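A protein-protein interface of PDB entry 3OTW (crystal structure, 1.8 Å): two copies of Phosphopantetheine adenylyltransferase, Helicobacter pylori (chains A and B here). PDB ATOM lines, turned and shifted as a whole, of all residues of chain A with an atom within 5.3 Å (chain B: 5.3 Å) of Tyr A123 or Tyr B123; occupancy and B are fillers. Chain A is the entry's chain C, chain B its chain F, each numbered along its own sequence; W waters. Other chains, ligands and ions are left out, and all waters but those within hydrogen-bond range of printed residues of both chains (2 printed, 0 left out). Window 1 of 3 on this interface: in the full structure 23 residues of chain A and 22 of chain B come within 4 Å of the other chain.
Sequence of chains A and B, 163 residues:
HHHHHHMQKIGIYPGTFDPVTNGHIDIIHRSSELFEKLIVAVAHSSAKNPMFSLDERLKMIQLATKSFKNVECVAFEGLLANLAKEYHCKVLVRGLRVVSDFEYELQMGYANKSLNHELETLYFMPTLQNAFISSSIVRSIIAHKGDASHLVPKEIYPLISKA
The backbone NH (N) of Arg A94 lies within hydrogen-bond range of the backbone carbonyl oxygen (O) of Leu A122, at 2.9 Å.
O of Arg A94 sits at hydrogen-bond distance from N of Phe A124.
The backbone carbonyl oxygen (O) of Phe A124 is in hydrogen-bond range of the backbone NH (N) of Leu A96 (2.8 Å).
N of Arg B94 is in hydrogen-bond range of O of Leu B122 (2.9 Å).
The backbone carbonyl oxygen (O) of Arg B94 lies within hydrogen-bond range of the backbone NH (N) of Phe B124, 2.9 Å away.
The backbone carbonyl oxygen of Glu B105 sits at hydrogen-bond distance from the side-chain hydroxyl of Tyr B123 (3.1 Å).
Tyr A123 touches just these residues of chain B: Leu B122, Tyr B123 and Met B125.
Of chain A, only Leu A122, Tyr A123 and Met A125 come within 4 Å of Tyr B123.
Of the printed residues of chain A, Leu B106 touches Leu A96 (3.8 Å) and Met A125 (3.7 Å).
Printed residues of chain B within 4 Å of Leu A106: Met B125 (3.6 Å).
Of the printed residues of chain A, Leu B122 touches Leu A122, Tyr A123 and Phe A124.
Printed residues of chain A within 4 Å of Phe B124: Leu A122.
Of the printed residues of chain B, Met A125 touches Leu B106 (3.7 Å) and Tyr B123 (3.3 Å).
The backbone NH (N) of Tyr B123 lies within hydrogen-bond range of the backbone carbonyl oxygen (O) of Tyr A123 (2.8 Å).
The side-chain hydroxyl of Tyr A123 lies within hydrogen-bond range of the side-chain sulfur of Met B125 (3.4 Å).
OH of Tyr B123 lies within hydrogen-bond range of SD of Met A125 (3.3 Å).
Leu A96 touches its own counterpart, Leu B96.
Leu A96 touches Leu B106, but with the chains exchanged Leu A106 does not touch Leu B96 (4.01 Å).
Leu A122 touches Tyr B123, and with the chains exchanged Tyr A123 touches Leu B122.
Tyr A123 touches Met B125, and with the chains exchanged Met A125 touches Tyr B123.
11 positions are printed for both chains.
Of the 12 pairs that touch across the chains among the printed residues, 11 have their exchanged pair printed and touching as well.
Water W1 lies within hydrogen-bond range of O of Thr A121 (2.6 Å) and N of Met B125 (2.8 Å).
Water W2 bridges the backbone carbonyl oxygen of Thr B121 (2.7 Å) and the backbone NH of Met A125 (2.9 Å).
Hydrophobic or aromatic side chains of chain B that line the printed part of chain A: Leu B96, Leu B106, Leu B122, Tyr B123, Phe B124 and Met B125.
Of the 11 printed residues of chain A, 6 touch a printed residue of chain B.
Hydrophobic or aromatic side chains of chain A that line the printed part of chain B: Leu A96, Leu A106, Leu A122, Tyr A123, Phe A124 and Met A125.
CD1 of Leu A96 touches CD1 of Leu B96, at 3.5 Å.
CD2 of Leu B106 touches O of Leu A96, at 3.8 Å.
O of Leu A106 touches CE of Met B125, 3.6 Å away.
Leu B122 touches Leu A122.
Leu A122 touches Tyr B123 (CA to O, 3.4 Å).
Leu A122 touches Phe B124.
Leu B122 touches Tyr A123.
CZ of Phe A124 touches CD1 of Leu B122, at 3.6 Å.
CE of Met A125 touches O of Leu B106, at 3.7 Å.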
ATOM      1  N   ARG A  94      18.858  26.541 -19.288  1.00  0.00           N
ATOM      2  CA  ARG A  94      18.082  27.122 -18.209  1.00  0.00           C
ATOM      3  C   ARG A  94      18.941  27.145 -16.950  1.00  0.00           C
ATOM      4  O   ARG A  94      19.860  26.356 -16.793  1.00  0.00           O
ATOM      5  CB  ARG A  94      16.782  26.337 -17.931  1.00  0.00           C
ATOM      6  CG  ARG A  94      15.797  26.314 -19.099  1.00  0.00           C
ATOM      7  CD  ARG A  94      15.096  27.628 -19.260  1.00  0.00           C
ATOM      8  NE  ARG A  94      14.174  27.855 -18.125  1.00  0.00           N
ATOM      9  CZ  ARG A  94      13.550  29.003 -17.912  1.00  0.00           C
ATOM     10  NH1 ARG A  94      13.709  30.013 -18.742  1.00  0.00           N
ATOM     11  NH2 ARG A  94      12.758  29.138 -16.853  1.00  0.00           N
ATOM     12  N   GLY A  95      18.648  28.080 -16.064  1.00  0.00           N
ATOM     13  CA  GLY A  95      19.378  28.128 -14.796  1.00  0.00           C
ATOM     14  C   GLY A  95      18.557  27.573 -13.673  1.00  0.00           C
ATOM     15  O   GLY A  95      17.338  27.712 -13.664  1.00  0.00           O
ATOM     16  N   LEU A  96      19.219  26.881 -12.751  1.00  0.00           N
ATOM     17  CA  LEU A  96      18.535  26.359 -11.582  1.00  0.00           C
ATOM     18  C   LEU A  96      19.069  27.079 -10.371  1.00  0.00           C
ATOM     19  O   LEU A  96      20.266  26.945 -10.046  1.00  0.00           O
ATOM     20  CB  LEU A  96      18.789  24.889 -11.445  1.00  0.00           C
ATOM     21  CG  LEU A  96      18.046  24.093 -12.495  1.00  0.00           C
ATOM     22  CD1 LEU A  96      18.351  22.670 -12.209  1.00  0.00           C
ATOM     23  CD2 LEU A  96      16.514  24.394 -12.507  1.00  0.00           C
ATOM     24  N   GLU A 105       9.962  23.460 -14.334  1.00  0.00           N
ATOM     25  CA  GLU A 105      11.061  23.379 -15.317  1.00  0.00           C
ATOM     26  C   GLU A 105      10.972  22.089 -16.143  1.00  0.00           C
ATOM     27  O   GLU A 105      11.126  22.139 -17.367  1.00  0.00           O
ATOM     28  CB  GLU A 105      12.439  23.470 -14.623  1.00  0.00           C
ATOM     29  CG  GLU A 105      12.789  24.885 -14.109  1.00  0.00           C
ATOM     30  CD  GLU A 105      12.992  25.897 -15.167  1.00  0.00           C
ATOM     31  OE1 GLU A 105      13.219  25.562 -16.359  1.00  0.00           O
ATOM     32  OE2 GLU A 105      12.911  27.100 -14.822  1.00  0.00           O
ATOM     33  N   LEU A 106      10.697  20.964 -15.486  1.00  0.00           N
ATOM     34  CA  LEU A 106      10.610  19.664 -16.162  1.00  0.00           C
ATOM     35  C   LEU A 106       9.434  19.780 -17.121  1.00  0.00           C
ATOM     36  O   LEU A 106       9.508  19.392 -18.293  1.00  0.00           O
ATOM     37  CB  LEU A 106      10.351  18.544 -15.159  1.00  0.00           C
ATOM     38  CG  LEU A 106      11.463  18.257 -14.144  1.00  0.00           C
ATOM     39  CD1 LEU A 106      11.169  16.988 -13.333  1.00  0.00           C
ATOM     40  CD2 LEU A 106      12.779  18.097 -14.929  1.00  0.00           C
ATOM     41  N   GLY A 109      10.319  21.857 -20.047  1.00  0.00           N
ATOM     42  CA  GLY A 109      11.244  21.122 -20.924  1.00  0.00           C
ATOM     43  C   GLY A 109      10.490  20.106 -21.770  1.00  0.00           C
ATOM     44  O   GLY A 109      10.766  19.980 -22.974  1.00  0.00           O
ATOM     45  N   THR A 121      16.528  20.230 -23.020  1.00  0.00           N
ATOM     46  CA  THR A 121      16.797  21.340 -22.088  1.00  0.00           C
ATOM     47  C   THR A 121      17.911  20.916 -21.146  1.00  0.00           C
ATOM     48  O   THR A 121      17.873  19.823 -20.623  1.00  0.00           O
ATOM     49  CB  THR A 121      15.508  21.736 -21.312  1.00  0.00           C
ATOM     50  OG1 THR A 121      14.539  22.162 -22.279  1.00  0.00           O
ATOM     51  CG2 THR A 121      15.803  22.877 -20.312  1.00  0.00           C
ATOM     52  N   LEU A 122      18.909  21.778 -20.961  1.00  0.00           N
ATOM     53  CA  LEU A 122      20.061  21.508 -20.074  1.00  0.00           C
ATOM     54  C   LEU A 122      20.091  22.596 -19.005  1.00  0.00           C
ATOM     55  O   LEU A 122      19.813  23.757 -19.331  1.00  0.00           O
ATOM     56  CB  LEU A 122      21.370  21.637 -20.890  1.00  0.00           C
ATOM     57  CG  LEU A 122      21.895  20.394 -21.615  1.00  0.00           C
ATOM     58  CD1 LEU A 122      20.835  19.658 -22.467  1.00  0.00           C
ATOM     59  CD2 LEU A 122      23.093  20.752 -22.462  1.00  0.00           C
ATOM     60  N   TYR A 123      20.482  22.261 -17.779  1.00  0.00           N
ATOM     61  CA  TYR A 123      20.431  23.227 -16.678  1.00  0.00           C
ATOM     62  C   TYR A 123      21.808  23.451 -16.097  1.00  0.00           C
ATOM     63  O   TYR A 123      22.562  22.506 -15.875  1.00  0.00           O
ATOM     64  CB  TYR A 123      19.509  22.753 -15.540  1.00  0.00           C
ATOM     65  CG  TYR A 123      18.110  22.445 -16.010  1.00  0.00           C
ATOM     66  CD1 TYR A 123      17.096  23.431 -15.942  1.00  0.00           C
ATOM     67  CD2 TYR A 123      17.791  21.198 -16.538  1.00  0.00           C
ATOM     68  CE1 TYR A 123      15.803  23.152 -16.384  1.00  0.00           C
ATOM     69  CE2 TYR A 123      16.501  20.914 -16.984  1.00  0.00           C
ATOM     70  CZ  TYR A 123      15.514  21.890 -16.869  1.00  0.00           C
ATOM     71  OH  TYR A 123      14.247  21.634 -17.340  1.00  0.00           O
ATOM     72  N   PHE A 124      22.072  24.713 -15.786  1.00  0.00           N
ATOM     73  CA  PHE A 124      23.315  25.159 -15.153  1.00  0.00           C
ATOM     74  C   PHE A 124      22.928  25.817 -13.818  1.00  0.00           C
ATOM     75  O   PHE A 124      21.756  26.207 -13.611  1.00  0.00           O
ATOM     76  CB  PHE A 124      23.961  26.246 -16.010  1.00  0.00           C
ATOM     77  CG  PHE A 124      24.530  25.750 -17.326  1.00  0.00           C
ATOM     78  CD1 PHE A 124      25.883  25.498 -17.449  1.00  0.00           C
ATOM     79  CD2 PHE A 124      23.684  25.501 -18.420  1.00  0.00           C
ATOM     80  CE1 PHE A 124      26.402  25.048 -18.672  1.00  0.00           C
ATOM     81  CE2 PHE A 124      24.193  25.046 -19.627  1.00  0.00           C
ATOM     82  CZ  PHE A 124      25.536  24.825 -19.753  1.00  0.00           C
ATOM     83  N   MET A 125      23.914  25.945 -12.925  1.00  0.00           N
ATOM     84  CA  MET A 125      23.727  26.606 -11.631  1.00  0.00           C
ATOM     85  C   MET A 125      24.481  27.932 -11.621  1.00  0.00           C
ATOM     86  O   MET A 125      25.589  28.018 -12.174  1.00  0.00           O
ATOM     87  CB  MET A 125      24.361  25.748 -10.511  1.00  0.00           C
ATOM     88  CG  MET A 125      23.884  24.319 -10.531  1.00  0.00           C
ATOM     89  SD  MET A 125      24.804  23.316  -9.347  1.00  0.00           S
ATOM     90  CE  MET A 125      24.946  24.481  -8.010  1.00  0.00           C
ATOM     91  N   ARG B  94      24.648  15.431 -14.264  1.00  0.00           N
ATOM     92  CA  ARG B  94      23.631  14.863 -13.366  1.00  0.00           C
ATOM     93  C   ARG B  94      22.286  14.743 -14.086  1.00  0.00           C
ATOM     94  O   ARG B  94      22.034  15.461 -15.047  1.00  0.00           O
ATOM     95  CB  ARG B  94      23.470  15.705 -12.070  1.00  0.00           C
ATOM     96  CG  ARG B  94      24.749  15.772 -11.228  1.00  0.00           C
ATOM     97  CD  ARG B  94      25.038  14.434 -10.567  1.00  0.00           C
ATOM     98  NE  ARG B  94      24.056  14.188  -9.489  1.00  0.00           N
ATOM     99  CZ  ARG B  94      23.867  13.020  -8.880  1.00  0.00           C
ATOM    100  NH1 ARG B  94      24.563  11.960  -9.237  1.00  0.00           N
ATOM    101  NH2 ARG B  94      22.946  12.905  -7.913  1.00  0.00           N
ATOM    102  N   GLY B  95      21.442  13.811 -13.647  1.00  0.00           N
ATOM    103  CA  GLY B  95      20.094  13.670 -14.246  1.00  0.00           C
ATOM    104  C   GLY B  95      19.067  14.272 -13.300  1.00  0.00           C
ATOM    105  O   GLY B  95      19.202  14.137 -12.082  1.00  0.00           O
ATOM    106  N   LEU B  96      18.066  14.962 -13.839  1.00  0.00           N
ATOM    107  CA  LEU B  96      16.989  15.541 -13.019  1.00  0.00           C
ATOM    108  C   LEU B  96      15.693  14.842 -13.402  1.00  0.00           C
ATOM    109  O   LEU B  96      15.232  14.941 -14.557  1.00  0.00           O
ATOM    110  CB  LEU B  96      16.851  17.029 -13.257  1.00  0.00           C
ATOM    111  CG  LEU B  96      17.965  17.891 -12.672  1.00  0.00           C
ATOM    112  CD1 LEU B  96      17.689  19.357 -12.955  1.00  0.00           C
ATOM    113  CD2 LEU B  96      18.132  17.635 -11.179  1.00  0.00           C
ATOM    114  N   GLU B 105      20.621  18.444  -4.910  1.00  0.00           N
ATOM    115  CA  GLU B 105      21.494  18.559  -6.095  1.00  0.00           C
ATOM    116  C   GLU B 105      22.288  19.851  -6.097  1.00  0.00           C
ATOM    117  O   GLU B 105      23.487  19.834  -6.357  1.00  0.00           O
ATOM    118  CB  GLU B 105      20.688  18.431  -7.391  1.00  0.00           C
ATOM    119  CG  GLU B 105      20.147  17.026  -7.571  1.00  0.00           C
ATOM    120  CD  GLU B 105      21.188  16.017  -7.970  1.00  0.00           C
ATOM    121  OE1 GLU B 105      22.309  16.379  -8.383  1.00  0.00           O
ATOM    122  OE2 GLU B 105      20.881  14.819  -7.858  1.00  0.00           O
ATOM    123  N   LEU B 106      21.647  20.962  -5.759  1.00  0.00           N
ATOM    124  CA  LEU B 106      22.346  22.249  -5.731  1.00  0.00           C
ATOM    125  C   LEU B 106      23.423  22.179  -4.642  1.00  0.00           C
ATOM    126  O   LEU B 106      24.576  22.579  -4.844  1.00  0.00           O
ATOM    127  CB  LEU B 106      21.369  23.395  -5.440  1.00  0.00           C
ATOM    128  CG  LEU B 106      20.281  23.630  -6.504  1.00  0.00           C
ATOM    129  CD1 LEU B 106      19.416  24.826  -6.061  1.00  0.00           C
ATOM    130  CD2 LEU B 106      20.834  23.808  -7.946  1.00  0.00           C
ATOM    131  N   GLY B 109      26.351  20.100  -5.796  1.00  0.00           N
ATOM    132  CA  GLY B 109      27.066  20.881  -6.823  1.00  0.00           C
ATOM    133  C   GLY B 109      27.995  21.897  -6.175  1.00  0.00           C
ATOM    134  O   GLY B 109      29.200  21.994  -6.519  1.00  0.00           O
ATOM    135  N   THR B 121      28.593  21.677 -12.432  1.00  0.00           N
ATOM    136  CA  THR B 121      27.652  20.578 -12.544  1.00  0.00           C
ATOM    137  C   THR B 121      26.591  21.041 -13.550  1.00  0.00           C
ATOM    138  O   THR B 121      26.076  22.152 -13.435  1.00  0.00           O
ATOM    139  CB  THR B 121      27.017  20.209 -11.164  1.00  0.00           C
ATOM    140  OG1 THR B 121      28.037  19.761 -10.259  1.00  0.00           O
ATOM    141  CG2 THR B 121      25.956  19.114 -11.314  1.00  0.00           C
ATOM    142  N   LEU B 122      26.265  20.177 -14.508  1.00  0.00           N
ATOM    143  CA  LEU B 122      25.277  20.457 -15.572  1.00  0.00           C
ATOM    144  C   LEU B 122      24.222  19.373 -15.453  1.00  0.00           C
ATOM    145  O   LEU B 122      24.572  18.220 -15.187  1.00  0.00           O
ATOM    146  CB  LEU B 122      26.015  20.325 -16.940  1.00  0.00           C
ATOM    147  CG  LEU B 122      25.304  20.293 -18.294  1.00  0.00           C
ATOM    148  CD1 LEU B 122      24.538  21.603 -18.534  1.00  0.00           C
ATOM    149  CD2 LEU B 122      26.315  20.115 -19.414  1.00  0.00           C
ATOM    150  N   TYR B 123      22.943  19.697 -15.680  1.00  0.00           N
ATOM    151  CA  TYR B 123      21.869  18.720 -15.504  1.00  0.00           C
ATOM    152  C   TYR B 123      21.092  18.467 -16.775  1.00  0.00           C
ATOM    153  O   TYR B 123      20.832  19.407 -17.576  1.00  0.00           O
ATOM    154  CB  TYR B 123      20.865  19.236 -14.479  1.00  0.00           C
ATOM    155  CG  TYR B 123      21.490  19.525 -13.139  1.00  0.00           C
ATOM    156  CD1 TYR B 123      21.536  18.538 -12.132  1.00  0.00           C
ATOM    157  CD2 TYR B 123      22.039  20.769 -12.876  1.00  0.00           C
ATOM    158  CE1 TYR B 123      22.122  18.815 -10.852  1.00  0.00           C
ATOM    159  CE2 TYR B 123      22.611  21.054 -11.612  1.00  0.00           C
ATOM    160  CZ  TYR B 123      22.639  20.080 -10.626  1.00  0.00           C
ATOM    161  OH  TYR B 123      23.219  20.389  -9.406  1.00  0.00           O
ATOM    162  N   PHE B 124      20.767  17.189 -16.953  1.00  0.00           N
ATOM    163  CA  PHE B 124      20.013  16.729 -18.123  1.00  0.00           C
ATOM    164  C   PHE B 124      18.745  16.106 -17.655  1.00  0.00           C
ATOM    165  O   PHE B 124      18.648  15.696 -16.496  1.00  0.00           O
ATOM    166  CB  PHE B 124      20.820  15.647 -18.881  1.00  0.00           C
ATOM    167  CG  PHE B 124      22.039  16.171 -19.596  1.00  0.00           C
ATOM    168  CD1 PHE B 124      22.002  16.391 -20.953  1.00  0.00           C
ATOM    169  CD2 PHE B 124      23.242  16.383 -18.896  1.00  0.00           C
ATOM    170  CE1 PHE B 124      23.140  16.872 -21.647  1.00  0.00           C
ATOM    171  CE2 PHE B 124      24.378  16.846 -19.564  1.00  0.00           C
ATOM    172  CZ  PHE B 124      24.328  17.068 -20.937  1.00  0.00           C
ATOM    173  N   MET B 125      17.763  15.996 -18.550  1.00  0.00           N
ATOM    174  CA  MET B 125      16.506  15.318 -18.210  1.00  0.00           C
ATOM    175  C   MET B 125      16.383  14.005 -18.967  1.00  0.00           C
ATOM    176  O   MET B 125      16.757  13.945 -20.139  1.00  0.00           O
ATOM    177  CB  MET B 125      15.336  16.197 -18.678  1.00  0.00           C
ATOM    178  CG  MET B 125      15.352  17.615 -18.206  1.00  0.00           C
ATOM    179  SD  MET B 125      14.064  18.640 -18.978  1.00  0.00           S
ATOM    180  CE  MET B 125      12.581  17.674 -18.810  1.00  0.00           C
HETATM  181  O   HOH W   1      18.069  17.271 -20.996  1.00  0.00           O
HETATM  182  O   HOH W   2      26.453  24.802 -13.699  1.00  0.00           O
